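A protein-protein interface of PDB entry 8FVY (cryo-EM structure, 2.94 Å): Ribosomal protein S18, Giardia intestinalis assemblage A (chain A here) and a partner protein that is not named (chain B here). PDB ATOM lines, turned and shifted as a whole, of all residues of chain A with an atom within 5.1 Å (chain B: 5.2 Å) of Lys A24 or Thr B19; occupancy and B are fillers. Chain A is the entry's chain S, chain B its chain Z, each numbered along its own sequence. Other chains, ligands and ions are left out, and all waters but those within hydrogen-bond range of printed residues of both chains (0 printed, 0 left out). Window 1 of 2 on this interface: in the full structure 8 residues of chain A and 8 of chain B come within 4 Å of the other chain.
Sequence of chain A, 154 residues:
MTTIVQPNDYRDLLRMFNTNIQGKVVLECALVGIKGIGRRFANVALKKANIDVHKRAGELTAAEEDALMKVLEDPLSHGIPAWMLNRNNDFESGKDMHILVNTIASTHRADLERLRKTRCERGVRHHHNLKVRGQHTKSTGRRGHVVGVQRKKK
Printed residues of chain B within 4 Å of Tyr A10: Leu B20. Of chain B, only Tyr B17 (3.1 Å) and Thr B19 (2.8 Å) come within 4 Å of Lys A24. Of the printed residues of chain B, Arg A56 touches Thr B19 (3.3 Å) and Leu B20 (3.8 Å). Printed residues of chain A within 4 Å of Tyr B17: Lys A24 (3.1 Å). Of the printed residues of chain A, Thr B19 touches Lys A24 (2.8 Å) and Arg A56 (3.3 Å). Printed residues of chain A within 4 Å of Leu B20: Tyr A10 and Arg A56. Phe B21 touches none of the printed residues of chain A. The nearest residue of chain B that does not touch Lys A24 is Pro B18 (4.7 Å). The nearest residue of chain A that does not touch Thr B19 is Gly A23 (4.5 Å).
The backbone carbonyl oxygen (O) of Lys A24 is in hydrogen-bond range of the side-chain hydroxyl (OG1) of Thr B19 (2.8 Å).
OH of Tyr A10 is in hydrogen-bond range of O of Gly A23 (2.5 Å). O of Lys A24 is in hydrogen-bond range of NH1 of Arg A56 (2.5 Å).
Among the printed residues, merely in contact across the chains: Lys A24 with Tyr B17, Arg A56 with Thr B19, Arg A56 with Leu B20 and Tyr A10 with Leu B20.
Hydrophobic or aromatic side chains of chain A that line the printed part of chain B: Tyr A10. Hydrophobic or aromatic side chains of chain B that line the printed part of chain A: Leu B20.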
ATOM      1  N   TYR A  10      17.508  -6.124 -13.967  1.00  0.00           N
ATOM      2  CA  TYR A  10      18.880  -6.593 -13.889  1.00  0.00           C
ATOM      3  C   TYR A  10      19.695  -5.709 -12.970  1.00  0.00           C
ATOM      4  O   TYR A  10      19.576  -4.483 -12.993  1.00  0.00           O
ATOM      5  CB  TYR A  10      19.496  -6.618 -15.273  1.00  0.00           C
ATOM      6  CG  TYR A  10      20.892  -7.178 -15.329  1.00  0.00           C
ATOM      7  CD1 TYR A  10      21.983  -6.374 -15.085  1.00  0.00           C
ATOM      8  CD2 TYR A  10      21.117  -8.499 -15.650  1.00  0.00           C
ATOM      9  CE1 TYR A  10      23.251  -6.873 -15.146  1.00  0.00           C
ATOM     10  CE2 TYR A  10      22.379  -9.003 -15.717  1.00  0.00           C
ATOM     11  CZ  TYR A  10      23.445  -8.190 -15.463  1.00  0.00           C
ATOM     12  OH  TYR A  10      24.713  -8.705 -15.528  1.00  0.00           O
ATOM     13  N   GLN A  22      29.114 -10.103  -9.103  1.00  0.00           N
ATOM     14  CA  GLN A  22      28.838  -9.634 -10.446  1.00  0.00           C
ATOM     15  C   GLN A  22      27.722 -10.436 -11.090  1.00  0.00           C
ATOM     16  O   GLN A  22      27.500 -11.607 -10.783  1.00  0.00           O
ATOM     17  CB  GLN A  22      30.082  -9.732 -11.310  1.00  0.00           C
ATOM     18  CG  GLN A  22      30.939 -10.901 -10.977  1.00  0.00           C
ATOM     19  CD  GLN A  22      31.900 -10.594  -9.858  1.00  0.00           C
ATOM     20  OE1 GLN A  22      31.579  -9.824  -8.954  1.00  0.00           O
ATOM     21  NE2 GLN A  22      33.076 -11.197  -9.900  1.00  0.00           N
ATOM     22  N   GLY A  23      27.047  -9.796 -12.031  1.00  0.00           N
ATOM     23  CA  GLY A  23      25.861 -10.334 -12.651  1.00  0.00           C
ATOM     24  C   GLY A  23      26.064 -10.881 -14.036  1.00  0.00           C
ATOM     25  O   GLY A  23      25.085 -11.040 -14.773  1.00  0.00           O
ATOM     26  N   LYS A  24      27.295 -11.147 -14.427  1.00  0.00           N
ATOM     27  CA  LYS A  24      27.588 -11.806 -15.679  1.00  0.00           C
ATOM     28  C   LYS A  24      27.936 -13.265 -15.484  1.00  0.00           C
ATOM     29  O   LYS A  24      27.959 -14.019 -16.458  1.00  0.00           O
ATOM     30  CB  LYS A  24      28.749 -11.110 -16.384  1.00  0.00           C
ATOM     31  CG  LYS A  24      29.994 -11.049 -15.550  1.00  0.00           C
ATOM     32  CD  LYS A  24      31.146 -10.375 -16.256  1.00  0.00           C
ATOM     33  CE  LYS A  24      31.556 -11.069 -17.523  1.00  0.00           C
ATOM     34  NZ  LYS A  24      32.055 -12.425 -17.270  1.00  0.00           N
ATOM     35  N   VAL A  25      28.197 -13.667 -14.265  1.00  0.00           N
ATOM     36  CA  VAL A  25      28.578 -15.023 -13.959  1.00  0.00           C
ATOM     37  C   VAL A  25      27.331 -15.844 -13.704  1.00  0.00           C
ATOM     38  O   VAL A  25      26.275 -15.326 -13.344  1.00  0.00           O
ATOM     39  CB  VAL A  25      29.513 -15.066 -12.745  1.00  0.00           C
ATOM     40  CG1 VAL A  25      30.237 -16.362 -12.699  1.00  0.00           C
ATOM     41  CG2 VAL A  25      30.480 -13.929 -12.789  1.00  0.00           C
ATOM     42  N   VAL A  26      27.450 -17.152 -13.903  1.00  0.00           N
ATOM     43  CA  VAL A  26      26.355 -18.021 -13.535  1.00  0.00           C
ATOM     44  C   VAL A  26      26.258 -18.065 -12.027  1.00  0.00           C
ATOM     45  O   VAL A  26      27.236 -17.853 -11.305  1.00  0.00           O
ATOM     46  CB  VAL A  26      26.514 -19.430 -14.120  1.00  0.00           C
ATOM     47  CG1 VAL A  26      26.660 -19.356 -15.595  1.00  0.00           C
ATOM     48  CG2 VAL A  26      27.671 -20.100 -13.520  1.00  0.00           C
ATOM     49  N   ARG A  56      22.091 -16.385 -14.944  1.00  0.00           N
ATOM     50  CA  ARG A  56      23.041 -15.335 -14.653  1.00  0.00           C
ATOM     51  C   ARG A  56      22.572 -14.572 -13.437  1.00  0.00           C
ATOM     52  O   ARG A  56      21.400 -14.219 -13.312  1.00  0.00           O
ATOM     53  CB  ARG A  56      23.198 -14.416 -15.851  1.00  0.00           C
ATOM     54  CG  ARG A  56      23.670 -15.106 -17.082  1.00  0.00           C
ATOM     55  CD  ARG A  56      25.084 -15.563 -16.957  1.00  0.00           C
ATOM     56  NE  ARG A  56      25.469 -16.396 -18.084  1.00  0.00           N
ATOM     57  CZ  ARG A  56      26.718 -16.714 -18.383  1.00  0.00           C
ATOM     58  NH1 ARG A  56      27.734 -16.226 -17.711  1.00  0.00           N
ATOM     59  NH2 ARG A  56      26.955 -17.524 -19.400  1.00  0.00           N
ATOM     60  N   TYR B  17      34.003  -8.671 -21.268  1.00  0.00           N
ATOM     61  CA  TYR B  17      32.853  -8.653 -22.145  1.00  0.00           C
ATOM     62  C   TYR B  17      31.630  -9.094 -21.361  1.00  0.00           C
ATOM     63  O   TYR B  17      31.744  -9.878 -20.415  1.00  0.00           O
ATOM     64  CB  TYR B  17      33.017  -9.577 -23.355  1.00  0.00           C
ATOM     65  CG  TYR B  17      34.285  -9.477 -24.141  1.00  0.00           C
ATOM     66  CD1 TYR B  17      34.455  -8.489 -25.078  1.00  0.00           C
ATOM     67  CD2 TYR B  17      35.278 -10.415 -24.000  1.00  0.00           C
ATOM     68  CE1 TYR B  17      35.598  -8.413 -25.823  1.00  0.00           C
ATOM     69  CE2 TYR B  17      36.422 -10.348 -24.738  1.00  0.00           C
ATOM     70  CZ  TYR B  17      36.580  -9.348 -25.651  1.00  0.00           C
ATOM     71  OH  TYR B  17      37.730  -9.279 -26.395  1.00  0.00           O
ATOM     72  N   PRO B  18      30.452  -8.611 -21.733  1.00  0.00           N
ATOM     73  CA  PRO B  18      29.242  -9.023 -21.032  1.00  0.00           C
ATOM     74  C   PRO B  18      28.803 -10.413 -21.440  1.00  0.00           C
ATOM     75  O   PRO B  18      29.281 -10.981 -22.422  1.00  0.00           O
ATOM     76  CB  PRO B  18      28.218  -7.976 -21.459  1.00  0.00           C
ATOM     77  CG  PRO B  18      28.687  -7.551 -22.768  1.00  0.00           C
ATOM     78  CD  PRO B  18      30.166  -7.538 -22.689  1.00  0.00           C
ATOM     79  N   THR B  19      27.880 -10.955 -20.655  1.00  0.00           N
ATOM     80  CA  THR B  19      27.221 -12.210 -20.955  1.00  0.00           C
ATOM     81  C   THR B  19      25.760 -12.047 -21.326  1.00  0.00           C
ATOM     82  O   THR B  19      25.162 -12.992 -21.847  1.00  0.00           O
ATOM     83  CB  THR B  19      27.312 -13.141 -19.756  1.00  0.00           C
ATOM     84  OG1 THR B  19      27.086 -12.398 -18.554  1.00  0.00           O
ATOM     85  CG2 THR B  19      28.661 -13.741 -19.698  1.00  0.00           C
ATOM     86  N   LEU B  20      25.172 -10.889 -21.060  1.00  0.00           N
ATOM     87  CA  LEU B  20      23.774 -10.623 -21.344  1.00  0.00           C
ATOM     88  C   LEU B  20      23.664  -9.298 -22.073  1.00  0.00           C
ATOM     89  O   LEU B  20      24.289  -8.312 -21.672  1.00  0.00           O
ATOM     90  CB  LEU B  20      22.974 -10.589 -20.058  1.00  0.00           C
ATOM     91  CG  LEU B  20      22.408 -11.929 -19.610  1.00  0.00           C
ATOM     92  CD1 LEU B  20      21.773 -11.838 -18.259  1.00  0.00           C
ATOM     93  CD2 LEU B  20      21.418 -12.435 -20.597  1.00  0.00           C
ATOM     94  N   PHE B  21      22.871  -9.273 -23.133  1.00  0.00           N
ATOM     95  CA  PHE B  21      22.751  -8.063 -23.923  1.00  0.00           C
ATOM     96  C   PHE B  21      21.852  -7.073 -23.206  1.00  0.00           C
ATOM     97  O   PHE B  21      20.746  -7.409 -22.781  1.00  0.00           O
ATOM     98  CB  PHE B  21      22.152  -8.357 -25.287  1.00  0.00           C
ATOM     99  CG  PHE B  21      23.128  -8.305 -26.387  1.00  0.00           C
ATOM    100  CD1 PHE B  21      23.867  -7.179 -26.623  1.00  0.00           C
ATOM    101  CD2 PHE B  21      23.248  -9.368 -27.242  1.00  0.00           C
ATOM    102  CE1 PHE B  21      24.758  -7.148 -27.650  1.00  0.00           C
ATOM    103  CE2 PHE B  21      24.120  -9.342 -28.274  1.00  0.00           C
ATOM    104  CZ  PHE B  21      24.876  -8.234 -28.486  1.00  0.00           C
ATOM    105  N   SER B  52      30.764 -12.279 -25.089  1.00  0.00           N
ATOM    106  CA  SER B  52      31.166 -13.644 -24.823  1.00  0.00           C
ATOM    107  C   SER B  52      30.519 -14.613 -25.806  1.00  0.00           C
ATOM    108  O   SER B  52      29.584 -14.282 -26.533  1.00  0.00           O
ATOM    109  CB  SER B  52      30.820 -14.038 -23.398  1.00  0.00           C
ATOM    110  OG  SER B  52      30.909 -15.435 -23.226  1.00  0.00           O
ATOM    111  N   LEU B  55      26.497 -16.020 -25.626  1.00  0.00           N
ATOM    112  CA  LEU B  55      25.474 -15.214 -26.256  1.00  0.00           C
ATOM    113  C   LEU B  55      25.435 -15.480 -27.740  1.00  0.00           C
ATOM    114  O   LEU B  55      24.360 -15.500 -28.352  1.00  0.00           O
ATOM    115  CB  LEU B  55      25.755 -13.755 -25.981  1.00  0.00           C
ATOM    116  CG  LEU B  55      24.983 -13.178 -24.817  1.00  0.00           C
ATOM    117  CD1 LEU B  55      25.504 -11.813 -24.445  1.00  0.00           C
ATOM    118  CD2 LEU B  55      23.569 -13.126 -25.225  1.00  0.00           C
